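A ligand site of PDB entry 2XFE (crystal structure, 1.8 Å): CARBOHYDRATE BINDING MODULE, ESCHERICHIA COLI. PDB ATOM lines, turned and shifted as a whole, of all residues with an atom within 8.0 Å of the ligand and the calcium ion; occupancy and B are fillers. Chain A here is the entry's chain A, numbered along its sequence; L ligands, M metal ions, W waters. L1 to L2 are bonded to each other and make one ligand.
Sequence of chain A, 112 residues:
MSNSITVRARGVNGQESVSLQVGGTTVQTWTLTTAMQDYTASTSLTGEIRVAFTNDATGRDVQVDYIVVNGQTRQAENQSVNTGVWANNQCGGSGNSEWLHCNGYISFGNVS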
ATOM      1  N   VAL A  12      24.499 -22.297 -14.077  1.00  0.00           N
ATOM      2  CA  VAL A  12      23.605 -23.424 -13.771  1.00  0.00           C
ATOM      3  C   VAL A  12      23.876 -23.956 -12.358  1.00  0.00           C
ATOM      4  O   VAL A  12      22.944 -24.319 -11.613  1.00  0.00           O
ATOM      5  CB  VAL A  12      23.797 -24.498 -14.884  1.00  0.00           C
ATOM      6  CG1 VAL A  12      23.293 -25.843 -14.412  1.00  0.00           C
ATOM      7  CG2 VAL A  12      23.161 -24.009 -16.198  1.00  0.00           C
ATOM      8  N   GLU A  16      30.445 -21.310 -11.615  1.00  0.00           N
ATOM      9  CA  GLU A  16      30.965 -20.872 -12.900  1.00  0.00           C
ATOM     10  C   GLU A  16      31.704 -19.556 -12.764  1.00  0.00           C
ATOM     11  O   GLU A  16      31.291 -18.690 -12.041  1.00  0.00           O
ATOM     12  CB  GLU A  16      29.814 -20.734 -13.939  1.00  0.00           C
ATOM     13  CG  GLU A  16      29.142 -22.025 -14.345  1.00  0.00           C
ATOM     14  CD  GLU A  16      27.960 -22.478 -13.459  1.00  0.00           C
ATOM     15  OE1 GLU A  16      27.659 -21.831 -12.414  1.00  0.00           O
ATOM     16  OE2 GLU A  16      27.324 -23.440 -13.864  1.00  0.00           O
ATOM     17  N   PHE A  53      33.849 -17.661 -20.297  1.00  0.00           N
ATOM     18  CA  PHE A  53      33.639 -18.730 -19.345  1.00  0.00           C
ATOM     19  C   PHE A  53      34.926 -19.573 -19.401  1.00  0.00           C
ATOM     20  O   PHE A  53      35.370 -20.002 -20.507  1.00  0.00           O
ATOM     21  CB  PHE A  53      32.445 -19.513 -19.797  1.00  0.00           C
ATOM     22  CG  PHE A  53      32.152 -20.735 -19.047  1.00  0.00           C
ATOM     23  CD1 PHE A  53      32.408 -20.886 -17.689  1.00  0.00           C
ATOM     24  CD2 PHE A  53      31.514 -21.771 -19.718  1.00  0.00           C
ATOM     25  CE1 PHE A  53      32.026 -22.056 -17.017  1.00  0.00           C
ATOM     26  CE2 PHE A  53      31.107 -22.934 -19.073  1.00  0.00           C
ATOM     27  CZ  PHE A  53      31.313 -23.080 -17.737  1.00  0.00           C
ATOM     28  N   ASN A  55      36.032 -22.080 -16.683  1.00  0.00           N
ATOM     29  CA  ASN A  55      36.149 -23.234 -15.767  1.00  0.00           C
ATOM     30  C   ASN A  55      35.069 -24.296 -16.030  1.00  0.00           C
ATOM     31  O   ASN A  55      34.535 -24.954 -15.120  1.00  0.00           O
ATOM     32  CB  ASN A  55      36.189 -22.733 -14.327  1.00  0.00           C
ATOM     33  CG  ASN A  55      34.873 -22.232 -13.817  1.00  0.00           C
ATOM     34  OD1 ASN A  55      34.036 -21.725 -14.578  1.00  0.00           O
ATOM     35  ND2 ASN A  55      34.705 -22.271 -12.516  1.00  0.00           N
ATOM     36  N   ASP A  56      34.753 -24.538 -17.311  1.00  0.00           N
ATOM     37  CA  ASP A  56      33.827 -25.588 -17.641  1.00  0.00           C
ATOM     38  C   ASP A  56      34.212 -26.891 -16.936  1.00  0.00           C
ATOM     39  O   ASP A  56      35.395 -27.228 -16.802  1.00  0.00           O
ATOM     40  CB  ASP A  56      33.738 -25.775 -19.134  1.00  0.00           C
ATOM     41  CG  ASP A  56      32.597 -26.633 -19.563  1.00  0.00           C
ATOM     42  OD1 ASP A  56      31.574 -26.560 -18.879  1.00  0.00           O
ATOM     43  OD2 ASP A  56      32.750 -27.343 -20.587  1.00  0.00           O
ATOM     44  N   ALA A  57      33.185 -27.610 -16.474  1.00  0.00           N
ATOM     45  CA  ALA A  57      33.334 -28.943 -15.812  1.00  0.00           C
ATOM     46  C   ALA A  57      31.961 -29.614 -15.911  1.00  0.00           C
ATOM     47  O   ALA A  57      30.966 -28.991 -16.266  1.00  0.00           O
ATOM     48  CB  ALA A  57      33.716 -28.772 -14.364  1.00  0.00           C
ATOM     49  N   THR A  58      31.909 -30.900 -15.588  1.00  0.00           N
ATOM     50  CA  THR A  58      30.674 -31.610 -15.601  1.00  0.00           C
ATOM     51  C   THR A  58      29.723 -30.850 -14.729  1.00  0.00           C
ATOM     52  O   THR A  58      29.983 -30.676 -13.576  1.00  0.00           O
ATOM     53  CB  THR A  58      30.900 -33.098 -15.156  1.00  0.00           C
ATOM     54  OG1 THR A  58      31.839 -33.704 -16.080  1.00  0.00           O
ATOM     55  CG2 THR A  58      29.569 -33.849 -15.203  1.00  0.00           C
ATOM     56  N   GLY A  59      28.612 -30.330 -15.304  1.00  0.00           N
ATOM     57  CA  GLY A  59      27.575 -29.639 -14.569  1.00  0.00           C
ATOM     58  C   GLY A  59      27.557 -28.081 -14.557  1.00  0.00           C
ATOM     59  O   GLY A  59      26.640 -27.478 -14.064  1.00  0.00           O
ATOM     60  N   ARG A  60      28.562 -27.455 -15.197  1.00  0.00           N
ATOM     61  CA  ARG A  60      28.699 -25.993 -15.215  1.00  0.00           C
ATOM     62  C   ARG A  60      28.365 -25.451 -16.652  1.00  0.00           C
ATOM     63  O   ARG A  60      28.876 -25.970 -17.601  1.00  0.00           O
ATOM     64  CB  ARG A  60      30.143 -25.587 -14.896  1.00  0.00           C
ATOM     65  CG  ARG A  60      30.601 -25.966 -13.461  1.00  0.00           C
ATOM     66  CD  ARG A  60      32.002 -25.488 -13.209  1.00  0.00           C
ATOM     67  NE  ARG A  60      32.500 -25.868 -11.912  1.00  0.00           N
ATOM     68  CZ  ARG A  60      33.756 -25.961 -11.581  1.00  0.00           C
ATOM     69  NH1 ARG A  60      34.713 -25.794 -12.473  1.00  0.00           N
ATOM     70  NH2 ARG A  60      34.036 -26.302 -10.322  1.00  0.00           N
ATOM     71  N   ASP A  61      27.573 -24.396 -16.739  1.00  0.00           N
ATOM     72  CA  ASP A  61      27.224 -23.682 -17.980  1.00  0.00           C
ATOM     73  C   ASP A  61      26.931 -22.242 -17.618  1.00  0.00           C
ATOM     74  O   ASP A  61      26.395 -21.998 -16.537  1.00  0.00           O
ATOM     75  CB  ASP A  61      25.940 -24.173 -18.655  1.00  0.00           C
ATOM     76  CG  ASP A  61      26.050 -25.580 -19.255  1.00  0.00           C
ATOM     77  OD1 ASP A  61      25.010 -26.249 -19.323  1.00  0.00           O
ATOM     78  OD2 ASP A  61      27.126 -25.953 -19.753  1.00  0.00           O
ATOM     79  N   VAL A  62      27.259 -21.307 -18.512  1.00  0.00           N
ATOM     80  CA  VAL A  62      27.056 -19.873 -18.267  1.00  0.00           C
ATOM     81  C   VAL A  62      26.005 -19.365 -19.222  1.00  0.00           C
ATOM     82  O   VAL A  62      25.935 -19.835 -20.391  1.00  0.00           O
ATOM     83  CB  VAL A  62      28.390 -19.106 -18.395  1.00  0.00           C
ATOM     84  CG1 VAL A  62      28.123 -17.606 -18.500  1.00  0.00           C
ATOM     85  CG2 VAL A  62      29.311 -19.435 -17.202  1.00  0.00           C
ATOM     86  N   GLY A  84      31.706 -20.568 -27.102  1.00  0.00           N
ATOM     87  CA  GLY A  84      31.377 -21.537 -26.075  1.00  0.00           C
ATOM     88  C   GLY A  84      30.010 -22.173 -26.166  1.00  0.00           C
ATOM     89  O   GLY A  84      29.785 -23.188 -25.560  1.00  0.00           O
ATOM     90  N   VAL A  85      29.116 -21.630 -26.982  1.00  0.00           N
ATOM     91  CA  VAL A  85      27.801 -22.215 -27.103  1.00  0.00           C
ATOM     92  C   VAL A  85      27.847 -23.636 -27.728  1.00  0.00           C
ATOM     93  O   VAL A  85      28.528 -23.866 -28.729  1.00  0.00           O
ATOM     94  CB  VAL A  85      26.905 -21.293 -27.949  1.00  0.00           C
ATOM     95  CG1 VAL A  85      27.474 -21.082 -29.358  1.00  0.00           C
ATOM     96  CG2 VAL A  85      25.442 -21.816 -27.999  1.00  0.00           C
ATOM     97  N   TRP A  86      27.110 -24.565 -27.168  1.00  0.00           N
ATOM     98  CA  TRP A  86      26.829 -25.851 -27.800  1.00  0.00           C
ATOM     99  C   TRP A  86      25.737 -25.684 -28.866  1.00  0.00           C
ATOM    100  O   TRP A  86      24.600 -25.346 -28.562  1.00  0.00           O
ATOM    101  CB  TRP A  86      26.374 -26.869 -26.762  1.00  0.00           C
ATOM    102  CG  TRP A  86      26.221 -28.222 -27.313  1.00  0.00           C
ATOM    103  CD1 TRP A  86      25.049 -28.855 -27.685  1.00  0.00           C
ATOM    104  CD2 TRP A  86      27.262 -29.131 -27.593  1.00  0.00           C
ATOM    105  NE1 TRP A  86      25.338 -30.129 -28.149  1.00  0.00           N
ATOM    106  CE2 TRP A  86      26.691 -30.302 -28.118  1.00  0.00           C
ATOM    107  CE3 TRP A  86      28.624 -29.094 -27.399  1.00  0.00           C
ATOM    108  CZ2 TRP A  86      27.431 -31.391 -28.452  1.00  0.00           C
ATOM    109  CZ3 TRP A  86      29.379 -30.211 -27.766  1.00  0.00           C
ATOM    110  CH2 TRP A  86      28.770 -31.308 -28.322  1.00  0.00           C
ATOM    111  N   ALA A  87      26.086 -25.891 -30.104  1.00  0.00           N
ATOM    112  CA  ALA A  87      25.150 -25.701 -31.197  1.00  0.00           C
ATOM    113  C   ALA A  87      25.709 -26.545 -32.364  1.00  0.00           C
ATOM    114  O   ALA A  87      26.927 -26.799 -32.478  1.00  0.00           O
ATOM    115  CB  ALA A  87      25.099 -24.261 -31.575  1.00  0.00           C
ATOM    116  N   ASN A  89      25.797 -29.527 -32.720  1.00  0.00           N
ATOM    117  CA  ASN A  89      26.447 -30.718 -32.129  1.00  0.00           C
ATOM    118  C   ASN A  89      27.949 -30.502 -31.855  1.00  0.00           C
ATOM    119  O   ASN A  89      28.794 -31.437 -32.062  1.00  0.00           O
ATOM    120  CB  ASN A  89      26.231 -31.956 -32.997  1.00  0.00           C
ATOM    121  CG  ASN A  89      26.502 -33.253 -32.249  1.00  0.00           C
ATOM    122  OD1 ASN A  89      25.889 -33.509 -31.219  1.00  0.00           O
ATOM    123  ND2 ASN A  89      27.381 -34.104 -32.807  1.00  0.00           N
ATOM    124  N   GLN A  90      28.295 -29.285 -31.435  1.00  0.00           N
ATOM    125  CA  GLN A  90      29.697 -28.956 -31.165  1.00  0.00           C
ATOM    126  C   GLN A  90      29.813 -27.701 -30.294  1.00  0.00           C
ATOM    127  O   GLN A  90      28.931 -26.881 -30.292  1.00  0.00           O
ATOM    128  CB  GLN A  90      30.469 -28.695 -32.473  1.00  0.00           C
ATOM    129  CG  GLN A  90      30.242 -27.333 -33.038  1.00  0.00           C
ATOM    130  CD  GLN A  90      31.154 -26.982 -34.217  1.00  0.00           C
ATOM    131  OE1 GLN A  90      32.013 -26.090 -34.145  1.00  0.00           O
ATOM    132  NE2 GLN A  90      30.921 -27.640 -35.305  1.00  0.00           N
ATOM    133  N   CYS A  91      30.943 -27.584 -29.605  1.00  0.00           N
ATOM    134  CA  CYS A  91      31.326 -26.403 -28.825  1.00  0.00           C
ATOM    135  C   CYS A  91      31.629 -25.271 -29.778  1.00  0.00           C
ATOM    136  O   CYS A  91      32.251 -25.500 -30.806  1.00  0.00           O
ATOM    137  CB  CYS A  91      32.607 -26.675 -28.014  1.00  0.00           C
ATOM    138  SG  CYS A  91      32.351 -27.829 -26.658  1.00  0.00           S
ATOM    139  N   TRP A  99      24.250 -18.393 -24.319  1.00  0.00           N
ATOM    140  CA  TRP A  99      24.853 -19.524 -23.598  1.00  0.00           C
ATOM    141  C   TRP A  99      26.309 -19.746 -23.908  1.00  0.00           C
ATOM    142  O   TRP A  99      26.745 -19.660 -25.070  1.00  0.00           O
ATOM    143  CB  TRP A  99      24.015 -20.779 -23.822  1.00  0.00           C
ATOM    144  CG  TRP A  99      22.709 -20.736 -23.079  1.00  0.00           C
ATOM    145  CD1 TRP A  99      21.550 -20.243 -23.553  1.00  0.00           C
ATOM    146  CD2 TRP A  99      22.460 -21.084 -21.700  1.00  0.00           C
ATOM    147  NE1 TRP A  99      20.599 -20.265 -22.588  1.00  0.00           N
ATOM    148  CE2 TRP A  99      21.118 -20.815 -21.450  1.00  0.00           C
ATOM    149  CE3 TRP A  99      23.223 -21.659 -20.694  1.00  0.00           C
ATOM    150  CZ2 TRP A  99      20.543 -21.030 -20.206  1.00  0.00           C
ATOM    151  CZ3 TRP A  99      22.644 -21.869 -19.471  1.00  0.00           C
ATOM    152  CH2 TRP A  99      21.341 -21.598 -19.233  1.00  0.00           C
ATOM    153  N   LEU A 100      27.088 -20.016 -22.861  1.00  0.00           N
ATOM    154  CA  LEU A 100      28.406 -20.580 -22.988  1.00  0.00           C
ATOM    155  C   LEU A 100      28.357 -21.918 -22.243  1.00  0.00           C
ATOM    156  O   LEU A 100      28.417 -21.951 -21.016  1.00  0.00           O
ATOM    157  CB  LEU A 100      29.457 -19.684 -22.369  1.00  0.00           C
ATOM    158  CG  LEU A 100      29.606 -18.338 -23.084  1.00  0.00           C
ATOM    159  CD1 LEU A 100      30.406 -17.301 -22.335  1.00  0.00           C
ATOM    160  CD2 LEU A 100      30.358 -18.573 -24.367  1.00  0.00           C
ATOM    161  N   HIS A 101      28.206 -22.991 -23.010  1.00  0.00           N
ATOM    162  CA  HIS A 101      28.167 -24.401 -22.482  1.00  0.00           C
ATOM    163  C   HIS A 101      29.570 -24.965 -22.311  1.00  0.00           C
ATOM    164  O   HIS A 101      29.853 -25.666 -21.345  1.00  0.00           O
ATOM    165  CB  HIS A 101      27.373 -25.353 -23.394  1.00  0.00           C
ATOM    166  CG  HIS A 101      25.983 -24.896 -23.683  1.00  0.00           C
ATOM    167  ND1 HIS A 101      24.928 -25.082 -22.815  1.00  0.00           N
ATOM    168  CD2 HIS A 101      25.487 -24.215 -24.750  1.00  0.00           C
ATOM    169  CE1 HIS A 101      23.840 -24.551 -23.321  1.00  0.00           C
ATOM    170  NE2 HIS A 101      24.152 -24.044 -24.512  1.00  0.00           N
ATOM    171  N   CYS A 102      30.457 -24.676 -23.253  1.00  0.00           N
ATOM    172  CA  CYS A 102      31.867 -25.020 -23.154  1.00  0.00           C
ATOM    173  C   CYS A 102      32.701 -23.778 -22.833  1.00  0.00           C
ATOM    174  O   CYS A 102      32.214 -22.629 -22.954  1.00  0.00           O
ATOM    175  CB  CYS A 102      32.302 -25.539 -24.524  1.00  0.00           C
ATOM    176  SG  CYS A 102      31.167 -26.809 -25.260  1.00  0.00           S
ATOM    177  N   ASN A 103      33.971 -23.984 -22.463  1.00  0.00           N
ATOM    178  CA  ASN A 103      34.865 -22.833 -22.298  1.00  0.00           C
ATOM    179  C   ASN A 103      34.931 -22.040 -23.596  1.00  0.00           C
ATOM    180  O   ASN A 103      34.954 -22.624 -24.671  1.00  0.00           O
ATOM    181  CB  ASN A 103      36.277 -23.256 -21.905  1.00  0.00           C
ATOM    182  CG  ASN A 103      36.376 -23.715 -20.455  1.00  0.00           C
ATOM    183  OD1 ASN A 103      35.674 -23.208 -19.563  1.00  0.00           O
ATOM    184  ND2 ASN A 103      37.271 -24.694 -20.223  1.00  0.00           N
HETATM  185  C1  LIG L   1      23.270 -31.758 -23.676  1.00  0.00           C
HETATM  186  C2  LIG L   1      23.630 -30.380 -23.218  1.00  0.00           C
HETATM  187  C3  LIG L   1      24.605 -29.712 -24.189  1.00  0.00           C
HETATM  188  C4  LIG L   1      25.864 -30.512 -24.346  1.00  0.00           C
HETATM  189  C5  LIG L   1      25.420 -31.954 -24.617  1.00  0.00           C
HETATM  190  C6  LIG L   1      26.579 -32.900 -24.815  1.00  0.00           C
HETATM  191  O1  LIG L   1      22.284 -32.265 -22.742  1.00  0.00           O
HETATM  192  O2  LIG L   1      22.460 -29.650 -23.199  1.00  0.00           O
HETATM  193  O3  LIG L   1      24.923 -28.458 -23.712  1.00  0.00           O
HETATM  194  O4  LIG L   1      26.574 -30.393 -23.090  1.00  0.00           O
HETATM  195  O5  LIG L   1      24.488 -32.453 -23.654  1.00  0.00           O
HETATM  196  O6  LIG L   1      25.996 -34.200 -24.926  1.00  0.00           O
HETATM  197  C1  LG2 L   2      27.970 -30.149 -23.196  1.00  0.00           C
HETATM  198  C2  LG2 L   2      28.592 -29.335 -22.020  1.00  0.00           C
HETATM  199  C3  LG2 L   2      30.086 -29.057 -22.038  1.00  0.00           C
HETATM  200  C4  LG2 L   2      30.889 -30.242 -22.609  1.00  0.00           C
HETATM  201  C5  LG2 L   2      30.167 -30.836 -23.852  1.00  0.00           C
HETATM  202  C6  LG2 L   2      30.915 -32.107 -24.332  1.00  0.00           C
HETATM  203  O1  LG2 L   2      27.852 -28.247 -21.480  1.00  0.00           O
HETATM  204  O2  LG2 L   2      30.484 -28.693 -20.708  1.00  0.00           O
HETATM  205  O3  LG2 L   2      31.072 -31.299 -21.663  1.00  0.00           O
HETATM  206  O4  LG2 L   2      28.775 -31.137 -23.784  1.00  0.00           O
HETATM  207  O5  LG2 L   2      30.626 -32.291 -25.669  1.00  0.00           O
HETATM  208 CA    CA M   1      29.138 -27.069 -19.615  1.00  0.00          CA
HETATM  209  O   HOH W   1      28.342 -28.863 -18.352  1.00  0.00           O
HETATM  210  O   HOH W   2      25.304 -28.486 -20.964  1.00  0.00           O
HETATM  211  O   HOH W   3      26.199 -32.387 -20.920  1.00  0.00           O
HETATM  212  O   HOH W   4      23.113 -27.009 -25.192  1.00  0.00           O
HETATM  213  O   HOH W   5      31.897 -30.605 -18.863  1.00  0.00           O
HETATM  214  O   HOH W   6      29.032 -33.125 -20.630  1.00  0.00           O
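Of the 23 residues printed, 4 come within 4 Å of the calcium ion.
The nearest printed residue that does not touch the calcium ion is Ala 57 (4.3 Å).
The calcium ion is bound by OD2 of Asp 61, O of Arg 60, water W1, O of His 101, O2 of LG2 L2, O1 of LG2 L2 and OD1 of Asp 56.
The side-chain carboxylate (OE2) of Glu 16 sits at hydrogen-bond distance from the backbone NH (N) of Asp 61.
The backbone carbonyl oxygen (O) of Asp 61 is in hydrogen-bond range of the backbone NH (N) of Val 12 (3.1 Å).
The guanidinium group (NH1) of Arg 60 lies within hydrogen-bond range of the backbone carbonyl oxygen (O) of Asn 55, at 2.8 Å.
The backbone carbonyl oxygen (O) of Gly 84 is in hydrogen-bond range of the backbone NH (N) of His 101.
The backbone NH (N) of Asp 56 is in hydrogen-bond range of the side-chain amide oxygen (OD1) of Asn 103 (2.8 Å).
SG of Cys 102 is disulfide-bonded to SG of Cys 91 (2.1 Å).
Merely in contact with the ligand: Trp 86.
Hydrophobic or aromatic side chains that line the ligand: Trp 86 and His 101.
Four residues have an atom within 4 Å of the ligand: Asp 56, Asp 61, Trp 86 and His 101.
Water W2 lies within hydrogen-bond range of an oxygen (O3) of LIG L1 (2.8 Å) and the side-chain carboxylate of Asp 61 (2.8 Å).
Water W4 bridges O3 of LIG L1 and NE2 of His 101.
Water W5 lies within hydrogen-bond range of an oxygen (O3) of LG2 L2, the backbone carbonyl oxygen of Ala 57 and the backbone NH of Thr 58.
ND1 of His 101 is in hydrogen-bond range of O3 of LIG L1, at 3.5 Å.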
